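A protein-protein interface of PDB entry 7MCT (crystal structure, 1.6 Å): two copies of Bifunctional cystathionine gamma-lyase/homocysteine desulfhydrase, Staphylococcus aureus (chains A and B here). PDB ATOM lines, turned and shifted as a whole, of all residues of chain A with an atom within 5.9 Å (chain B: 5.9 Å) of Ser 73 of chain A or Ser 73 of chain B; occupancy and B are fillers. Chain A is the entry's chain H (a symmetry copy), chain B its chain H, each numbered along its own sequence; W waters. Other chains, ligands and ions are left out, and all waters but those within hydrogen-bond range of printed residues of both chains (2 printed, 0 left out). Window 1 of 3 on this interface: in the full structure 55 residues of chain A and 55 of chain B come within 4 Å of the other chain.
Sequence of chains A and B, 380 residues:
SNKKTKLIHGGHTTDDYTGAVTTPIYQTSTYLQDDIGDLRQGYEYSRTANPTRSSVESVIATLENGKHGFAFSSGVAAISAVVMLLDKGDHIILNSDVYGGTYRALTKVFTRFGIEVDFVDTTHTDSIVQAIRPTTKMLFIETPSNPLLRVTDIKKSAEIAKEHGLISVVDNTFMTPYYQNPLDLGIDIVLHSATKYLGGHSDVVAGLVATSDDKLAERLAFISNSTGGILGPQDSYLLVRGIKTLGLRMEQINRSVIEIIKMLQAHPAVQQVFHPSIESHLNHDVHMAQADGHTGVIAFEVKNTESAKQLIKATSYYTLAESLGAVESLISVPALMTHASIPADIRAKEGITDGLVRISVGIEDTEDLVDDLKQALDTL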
ATOM      1  N   ALA A  71      -8.107 -19.790 -24.368  1.00  0.00           N
ATOM      2  CA  ALA A  71      -8.894 -19.120 -23.341  1.00  0.00           C
ATOM      3  C   ALA A  71      -9.137 -17.668 -23.729  1.00  0.00           C
ATOM      4  O   ALA A  71      -8.189 -16.921 -24.001  1.00  0.00           O
ATOM      5  CB  ALA A  71      -8.198 -19.197 -21.975  1.00  0.00           C
ATOM      6  N   PHE A  72     -10.409 -17.273 -23.743  1.00  0.00           N
ATOM      7  CA  PHE A  72     -10.849 -15.955 -24.166  1.00  0.00           C
ATOM      8  C   PHE A  72     -11.510 -15.212 -23.008  1.00  0.00           C
ATOM      9  O   PHE A  72     -11.947 -15.809 -22.017  1.00  0.00           O
ATOM     10  CB  PHE A  72     -11.826 -16.057 -25.353  1.00  0.00           C
ATOM     11  CG  PHE A  72     -11.192 -16.587 -26.612  1.00  0.00           C
ATOM     12  CD1 PHE A  72     -10.578 -15.724 -27.506  1.00  0.00           C
ATOM     13  CD2 PHE A  72     -11.184 -17.949 -26.883  1.00  0.00           C
ATOM     14  CE1 PHE A  72      -9.987 -16.205 -28.691  1.00  0.00           C
ATOM     15  CE2 PHE A  72     -10.594 -18.433 -28.060  1.00  0.00           C
ATOM     16  CZ  PHE A  72      -9.994 -17.560 -28.950  1.00  0.00           C
ATOM     17  N   SER A  73     -11.613 -13.891 -23.173  1.00  0.00           N
ATOM     18  CA  SER A  73     -12.131 -13.009 -22.135  1.00  0.00           C
ATOM     19  C   SER A  73     -13.610 -13.230 -21.825  1.00  0.00           C
ATOM     20  O   SER A  73     -14.109 -12.657 -20.849  1.00  0.00           O
ATOM     21  CB  SER A  73     -11.893 -11.558 -22.553  1.00  0.00           C
ATOM     22  OG  SER A  73     -12.370 -11.343 -23.880  1.00  0.00           O
ATOM     23  N   SER A  74     -14.318 -14.030 -22.620  1.00  0.00           N
ATOM     24  CA  SER A  74     -15.733 -14.310 -22.409  1.00  0.00           C
ATOM     25  C   SER A  74     -16.136 -15.411 -23.379  1.00  0.00           C
ATOM     26  O   SER A  74     -15.443 -15.670 -24.366  1.00  0.00           O
ATOM     27  CB  SER A  74     -16.587 -13.052 -22.615  1.00  0.00           C
ATOM     28  OG  SER A  74     -16.531 -12.622 -23.975  1.00  0.00           O
ATOM     29  N   GLY A  75     -17.269 -16.059 -23.089  1.00  0.00           N
ATOM     30  CA  GLY A  75     -17.850 -16.976 -24.067  1.00  0.00           C
ATOM     31  C   GLY A  75     -18.104 -16.340 -25.426  1.00  0.00           C
ATOM     32  O   GLY A  75     -17.813 -16.943 -26.472  1.00  0.00           O
ATOM     33  N   ALA A  77     -16.566 -13.864 -26.730  1.00  0.00           N
ATOM     34  CA  ALA A  77     -15.284 -13.632 -27.397  1.00  0.00           C
ATOM     35  C   ALA A  77     -14.755 -14.910 -28.038  1.00  0.00           C
ATOM     36  O   ALA A  77     -14.161 -14.863 -29.122  1.00  0.00           O
ATOM     37  CB  ALA A  77     -14.263 -13.051 -26.410  1.00  0.00           C
ATOM     38  N   ALA A  78     -14.982 -16.062 -27.402  1.00  0.00           N
ATOM     39  CA  ALA A  78     -14.610 -17.331 -28.023  1.00  0.00           C
ATOM     40  C   ALA A  78     -15.420 -17.562 -29.289  1.00  0.00           C
ATOM     41  O   ALA A  78     -14.879 -17.959 -30.333  1.00  0.00           O
ATOM     42  CB  ALA A  78     -14.829 -18.480 -27.044  1.00  0.00           C
ATOM     43  N   VAL A 205     -15.838 -14.364 -15.838  1.00  0.00           N
ATOM     44  CA  VAL A 205     -16.385 -14.329 -17.192  1.00  0.00           C
ATOM     45  C   VAL A 205     -15.271 -14.785 -18.130  1.00  0.00           C
ATOM     46  O   VAL A 205     -14.182 -14.200 -18.129  1.00  0.00           O
ATOM     47  CB  VAL A 205     -16.891 -12.927 -17.567  1.00  0.00           C
ATOM     48  CG1 VAL A 205     -17.287 -12.875 -19.045  1.00  0.00           C
ATOM     49  CG2 VAL A 205     -18.076 -12.516 -16.690  1.00  0.00           C
ATOM     50  N   ALA A 206     -15.536 -15.820 -18.929  1.00  0.00           N
ATOM     51  CA  ALA A 206     -14.464 -16.443 -19.705  1.00  0.00           C
ATOM     52  C   ALA A 206     -15.051 -17.379 -20.752  1.00  0.00           C
ATOM     53  O   ALA A 206     -16.126 -17.949 -20.559  1.00  0.00           O
ATOM     54  CB  ALA A 206     -13.503 -17.230 -18.794  1.00  0.00           C
ATOM     55  N   GLY A 207     -14.315 -17.549 -21.849  1.00  0.00           N
ATOM     56  CA  GLY A 207     -14.645 -18.552 -22.846  1.00  0.00           C
ATOM     57  C   GLY A 207     -13.477 -19.513 -23.038  1.00  0.00           C
ATOM     58  O   GLY A 207     -12.324 -19.152 -22.820  1.00  0.00           O
ATOM     59  N   THR A 227      -6.638 -10.073 -32.545  1.00  0.00           N
ATOM     60  CA  THR A 227      -7.770  -9.309 -32.027  1.00  0.00           C
ATOM     61  C   THR A 227      -7.823  -9.289 -30.498  1.00  0.00           C
ATOM     62  O   THR A 227      -8.584  -8.500 -29.936  1.00  0.00           O
ATOM     63  CB  THR A 227      -9.099  -9.842 -32.595  1.00  0.00           C
ATOM     64  OG1 THR A 227      -9.275 -11.225 -32.261  1.00  0.00           O
ATOM     65  CG2 THR A 227      -9.121  -9.700 -34.131  1.00  0.00           C
ATOM     66  N   GLY A 228      -7.057 -10.144 -29.826  1.00  0.00           N
ATOM     67  CA  GLY A 228      -6.690  -9.907 -28.432  1.00  0.00           C
ATOM     68  C   GLY A 228      -7.756 -10.093 -27.374  1.00  0.00           C
ATOM     69  O   GLY A 228      -7.623  -9.523 -26.283  1.00  0.00           O
ATOM     70  N   GLY A 229      -8.784 -10.898 -27.635  1.00  0.00           N
ATOM     71  CA  GLY A 229      -9.783 -11.183 -26.622  1.00  0.00           C
ATOM     72  C   GLY A 229      -9.341 -12.273 -25.664  1.00  0.00           C
ATOM     73  O   GLY A 229     -10.045 -13.270 -25.489  1.00  0.00           O
ATOM     74  N   ILE A 230      -8.175 -12.087 -25.012  1.00  0.00           N
ATOM     75  CA  ILE A 230      -7.553 -13.127 -24.196  1.00  0.00           C
ATOM     76  C   ILE A 230      -8.058 -13.070 -22.759  1.00  0.00           C
ATOM     77  O   ILE A 230      -8.381 -12.005 -22.223  1.00  0.00           O
ATOM     78  CB  ILE A 230      -6.016 -12.992 -24.235  1.00  0.00           C
ATOM     79  CG1 ILE A 230      -5.608 -11.601 -23.721  1.00  0.00           C
ATOM     80  CG2 ILE A 230      -5.512 -13.205 -25.654  1.00  0.00           C
ATOM     81  CD1 ILE A 230      -4.238 -11.535 -23.131  1.00  0.00           C
ATOM     82  N   LEU A 231      -8.102 -14.235 -22.128  1.00  0.00           N
ATOM     83  CA  LEU A 231      -8.375 -14.318 -20.695  1.00  0.00           C
ATOM     84  C   LEU A 231      -7.132 -13.939 -19.901  1.00  0.00           C
ATOM     85  O   LEU A 231      -6.024 -14.397 -20.206  1.00  0.00           O
ATOM     86  CB  LEU A 231      -8.822 -15.734 -20.328  1.00  0.00           C
ATOM     87  CG  LEU A 231      -9.426 -15.903 -18.923  1.00  0.00           C
ATOM     88  CD1 LEU A 231     -10.675 -15.041 -18.812  1.00  0.00           C
ATOM     89  CD2 LEU A 231      -9.746 -17.362 -18.629  1.00  0.00           C
ATOM     90  N   GLY A 232      -7.320 -13.129 -18.850  1.00  0.00           N
ATOM     91  CA  GLY A 232      -6.216 -12.747 -17.986  1.00  0.00           C
ATOM     92  C   GLY A 232      -5.807 -13.862 -17.042  1.00  0.00           C
ATOM     93  O   GLY A 232      -6.481 -14.894 -16.897  1.00  0.00           O
ATOM     94  N   ALA B  71     -12.945  -0.497 -21.221  1.00  0.00           N
ATOM     95  CA  ALA B  71     -11.760  -1.285 -20.910  1.00  0.00           C
ATOM     96  C   ALA B  71     -11.836  -2.643 -21.596  1.00  0.00           C
ATOM     97  O   ALA B  71     -12.815  -3.381 -21.426  1.00  0.00           O
ATOM     98  CB  ALA B  71     -11.598  -1.464 -19.394  1.00  0.00           C
ATOM     99  N   PHE B  72     -10.797  -2.968 -22.362  1.00  0.00           N
ATOM    100  CA  PHE B  72     -10.721  -4.179 -23.162  1.00  0.00           C
ATOM    101  C   PHE B  72      -9.574  -5.066 -22.687  1.00  0.00           C
ATOM    102  O   PHE B  72      -8.640  -4.616 -22.011  1.00  0.00           O
ATOM    103  CB  PHE B  72     -10.541  -3.839 -24.655  1.00  0.00           C
ATOM    104  CG  PHE B  72     -11.731  -3.144 -25.262  1.00  0.00           C
ATOM    105  CD1 PHE B  72     -12.773  -3.880 -25.805  1.00  0.00           C
ATOM    106  CD2 PHE B  72     -11.820  -1.759 -25.262  1.00  0.00           C
ATOM    107  CE1 PHE B  72     -13.889  -3.243 -26.382  1.00  0.00           C
ATOM    108  CE2 PHE B  72     -12.930  -1.119 -25.832  1.00  0.00           C
ATOM    109  CZ  PHE B  72     -13.959  -1.865 -26.381  1.00  0.00           C
ATOM    110  N   SER B  73      -9.641  -6.337 -23.091  1.00  0.00           N
ATOM    111  CA  SER B  73      -8.684  -7.348 -22.660  1.00  0.00           C
ATOM    112  C   SER B  73      -7.266  -7.109 -23.172  1.00  0.00           C
ATOM    113  O   SER B  73      -6.345  -7.808 -22.731  1.00  0.00           O
ATOM    114  CB  SER B  73      -9.181  -8.723 -23.109  1.00  0.00           C
ATOM    115  OG  SER B  73      -9.512  -8.698 -24.497  1.00  0.00           O
ATOM    116  N   SER B  74      -7.066  -6.159 -24.083  1.00  0.00           N
ATOM    117  CA  SER B  74      -5.751  -5.849 -24.632  1.00  0.00           C
ATOM    118  C   SER B  74      -5.888  -4.588 -25.473  1.00  0.00           C
ATOM    119  O   SER B  74      -6.992  -4.206 -25.868  1.00  0.00           O
ATOM    120  CB  SER B  74      -5.208  -7.014 -25.469  1.00  0.00           C
ATOM    121  OG  SER B  74      -6.014  -7.221 -26.628  1.00  0.00           O
ATOM    122  N   GLY B  75      -4.749  -3.942 -25.744  1.00  0.00           N
ATOM    123  CA  GLY B  75      -4.749  -2.851 -26.718  1.00  0.00           C
ATOM    124  C   GLY B  75      -5.305  -3.247 -28.078  1.00  0.00           C
ATOM    125  O   GLY B  75      -6.087  -2.498 -28.685  1.00  0.00           O
ATOM    126  N   ALA B  77      -7.422  -5.551 -28.717  1.00  0.00           N
ATOM    127  CA  ALA B  77      -8.869  -5.734 -28.608  1.00  0.00           C
ATOM    128  C   ALA B  77      -9.600  -4.396 -28.643  1.00  0.00           C
ATOM    129  O   ALA B  77     -10.688  -4.295 -29.221  1.00  0.00           O
ATOM    130  CB  ALA B  77      -9.217  -6.515 -27.334  1.00  0.00           C
ATOM    131  N   ALA B  78      -9.009  -3.352 -28.056  1.00  0.00           N
ATOM    132  CA  ALA B  78      -9.596  -2.019 -28.161  1.00  0.00           C
ATOM    133  C   ALA B  78      -9.594  -1.548 -29.607  1.00  0.00           C
ATOM    134  O   ALA B  78     -10.595  -1.015 -30.109  1.00  0.00           O
ATOM    135  CB  ALA B  78      -8.827  -1.033 -27.288  1.00  0.00           C
ATOM    136  N   VAL B 205      -2.092  -6.851 -19.266  1.00  0.00           N
ATOM    137  CA  VAL B 205      -2.371  -6.641 -20.685  1.00  0.00           C
ATOM    138  C   VAL B 205      -3.792  -6.094 -20.779  1.00  0.00           C
ATOM    139  O   VAL B 205      -4.733  -6.723 -20.281  1.00  0.00           O
ATOM    140  CB  VAL B 205      -2.217  -7.938 -21.494  1.00  0.00           C
ATOM    141  CG1 VAL B 205      -2.691  -7.732 -22.936  1.00  0.00           C
ATOM    142  CG2 VAL B 205      -0.767  -8.428 -21.481  1.00  0.00           C
ATOM    143  N   ALA B 206      -3.955  -4.932 -21.414  1.00  0.00           N
ATOM    144  CA  ALA B 206      -5.245  -4.244 -21.371  1.00  0.00           C
ATOM    145  C   ALA B 206      -5.275  -3.124 -22.401  1.00  0.00           C
ATOM    146  O   ALA B 206      -4.243  -2.541 -22.734  1.00  0.00           O
ATOM    147  CB  ALA B 206      -5.517  -3.661 -19.971  1.00  0.00           C
ATOM    148  N   GLY B 207      -6.481  -2.814 -22.878  1.00  0.00           N
ATOM    149  CA  GLY B 207      -6.697  -1.649 -23.716  1.00  0.00           C
ATOM    150  C   GLY B 207      -7.735  -0.727 -23.086  1.00  0.00           C
ATOM    151  O   GLY B 207      -8.600  -1.173 -22.338  1.00  0.00           O
ATOM    152  N   THR B 227     -19.084  -8.827 -28.729  1.00  0.00           N
ATOM    153  CA  THR B 227     -17.891  -9.609 -29.040  1.00  0.00           C
ATOM    154  C   THR B 227     -17.017  -9.873 -27.812  1.00  0.00           C
ATOM    155  O   THR B 227     -16.111 -10.705 -27.889  1.00  0.00           O
ATOM    156  CB  THR B 227     -17.059  -8.928 -30.144  1.00  0.00           C
ATOM    157  OG1 THR B 227     -16.664  -7.611 -29.741  1.00  0.00           O
ATOM    158  CG2 THR B 227     -17.882  -8.819 -31.445  1.00  0.00           C
ATOM    159  N   GLY B 228     -17.252  -9.175 -26.704  1.00  0.00           N
ATOM    160  CA  GLY B 228     -16.815  -9.652 -25.395  1.00  0.00           C
ATOM    161  C   GLY B 228     -15.338  -9.587 -25.072  1.00  0.00           C
ATOM    162  O   GLY B 228     -14.884 -10.332 -24.192  1.00  0.00           O
ATOM    163  N   GLY B 229     -14.579  -8.703 -25.715  1.00  0.00           N
ATOM    164  CA  GLY B 229     -13.177  -8.537 -25.377  1.00  0.00           C
ATOM    165  C   GLY B 229     -12.975  -7.639 -24.172  1.00  0.00           C
ATOM    166  O   GLY B 229     -12.242  -6.650 -24.249  1.00  0.00           O
ATOM    167  N   ILE B 230     -13.608  -7.983 -23.032  1.00  0.00           N
ATOM    168  CA  ILE B 230     -13.637  -7.120 -21.854  1.00  0.00           C
ATOM    169  C   ILE B 230     -12.436  -7.384 -20.953  1.00  0.00           C
ATOM    170  O   ILE B 230     -11.925  -8.504 -20.859  1.00  0.00           O
ATOM    171  CB  ILE B 230     -14.952  -7.320 -21.072  1.00  0.00           C
ATOM    172  CG1 ILE B 230     -15.082  -8.793 -20.652  1.00  0.00           C
ATOM    173  CG2 ILE B 230     -16.135  -6.906 -21.934  1.00  0.00           C
ATOM    174  CD1 ILE B 230     -15.913  -9.020 -19.432  1.00  0.00           C
ATOM    175  N   LEU B 231     -12.000  -6.334 -20.268  1.00  0.00           N
ATOM    176  CA  LEU B 231     -10.988  -6.471 -19.222  1.00  0.00           C
ATOM    177  C   LEU B 231     -11.618  -7.032 -17.955  1.00  0.00           C
ATOM    178  O   LEU B 231     -12.690  -6.585 -17.530  1.00  0.00           O
ATOM    179  CB  LEU B 231     -10.347  -5.113 -18.934  1.00  0.00           C
ATOM    180  CG  LEU B 231      -9.069  -5.144 -18.077  1.00  0.00           C
ATOM    181  CD1 LEU B 231      -8.003  -5.952 -18.803  1.00  0.00           C
ATOM    182  CD2 LEU B 231      -8.571  -3.738 -17.774  1.00  0.00           C
ATOM    183  N   GLY B 232     -10.929  -7.992 -17.321  1.00  0.00           N
ATOM    184  CA  GLY B 232     -11.403  -8.560 -16.071  1.00  0.00           C
ATOM    185  C   GLY B 232     -11.179  -7.634 -14.891  1.00  0.00           C
ATOM    186  O   GLY B 232     -10.486  -6.607 -14.971  1.00  0.00           O
HETATM  187  O   HOH W   1      -7.418  -9.876 -20.606  1.00  0.00           O
HETATM  188  O   HOH W   2     -11.956 -10.910 -19.347  1.00  0.00           O
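Ser 73 of chain A touches its own counterpart, Ser 73 of chain B. Ser 73 of chain A touches Gly 228 of chain B, and with the chains exchanged Gly 228 of chain A touches Ser 73 of chain B. Ser 73 of chain A touches Ile 230 of chain B, and with the chains exchanged Ile 230 of chain A touches Ser 73 of chain B. Ala 77 of chain A touches Gly 228 of chain B, and with the chains exchanged Gly 228 of chain A touches Ala 77 of chain B. Positions printed for both chains: 71, 72, 73, 74, 75, 77, 78, 205, 206, 207, 227, 228, 229, 230, 231 and 232. Of the 13 pairs that touch across the chains among the printed residues, 13 have their exchanged pair printed and touching as well.
O of Gly 229 of chain B lies within hydrogen-bond range of N of Ser 73 of chain B, at 2.9 Å. The backbone NH of Ala 77 of chain B is in hydrogen-bond range of the side-chain hydroxyl of Ser 74 of chain B, 3.0 Å away. The backbone carbonyl oxygen (O) of Ser 74 of chain B sits close to the backbone NH (N) of Gly 207 of chain B (3.3 Å). The backbone NH (N) of Ser 73 of chain A sits at hydrogen-bond distance from the backbone carbonyl oxygen (O) of Gly 229 of chain A (2.9 Å). The side-chain hydroxyl of Ser 74 of chain A sits at hydrogen-bond distance from the backbone NH of Ala 77 of chain A. The backbone NH (N) of Gly 207 of chain A sits close to the backbone carbonyl oxygen (O) of Ser 74 of chain A, 3.3 Å away.
Ser 73 of chain A touches four residues of chain B. Of the printed residues of chain A, Ser 74 of chain B touches Gly 228. Of the printed residues of chain A, Ala 77 of chain B touches Thr 227 and Gly 228. The nearest residue of chain B that does not touch Ser 73 of chain A is Thr 227 of chain B (5.5 Å). The nearest residue of chain A that does not touch Ser 73 of chain B is Thr 227 of chain A (5.5 Å).
The backbone carbonyl oxygen (O) of Gly 228 of chain A lies within hydrogen-bond range of the side-chain hydroxyl (OG) of Ser 73 of chain B (2.7 Å). The backbone carbonyl oxygen of Gly 228 of chain A lies within hydrogen-bond range of the side-chain hydroxyl of Ser 74 of chain B (2.8 Å). The backbone NH (N) of Ala 77 of chain B sits close to the backbone carbonyl oxygen (O) of Thr 227 of chain A, at 3.4 Å. O of Thr 227 of chain B sits close to N of Ala 77 of chain A (3.4 Å). O of Gly 228 of chain B lies within hydrogen-bond range of OG of Ser 73 of chain A, at 2.7 Å. The side-chain hydroxyl (OG) of Ser 74 of chain A is in hydrogen-bond range of the backbone carbonyl oxygen (O) of Gly 228 of chain B.
Of the 16 printed residues of chain A, 7 touch a printed residue of chain B. Hydrophobic or aromatic side chains of chain A that line the printed part of chain B: Ala 77 and Ile 230. Of the 16 printed residues of chain B, 7 touch a printed residue of chain A. Along chain B the printed residues that touch a printed residue of chain A span positions 73 to 230. Among the printed residues, 13 pairs touch across the chains. Among the printed residues, no Asp or Glu carboxylate lies within 4 Å of a Lys or Arg side-chain nitrogen of the other chain.
Among the printed residues, merely in contact across the chains: Ser 73 of chain A with Ser 73 of chain B (3.9 Å), Ser 73 of chain A with Gly 229 of chain B (3.3 Å), Ser 73 of chain A with Ile 230 of chain B (3.5 Å), Ala 77 of chain A with Gly 228 of chain B (3.6 Å), Gly 228 of chain A with Ala 77 of chain B (3.6 Å), Gly 229 of chain A with Ser 73 of chain B (3.3 Å) and Ile 230 of chain A with Ser 73 of chain B (3.5 Å).
Water W2 lies within hydrogen-bond range of O of Ile 230 of chain B and O of Ser 73 of chain A. Water W1 lies within hydrogen-bond range of the backbone carbonyl oxygen (O) of Ile 230 of chain A (2.8 Å) and the backbone carbonyl oxygen (O) of Ser 73 of chain B (3.2 Å).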
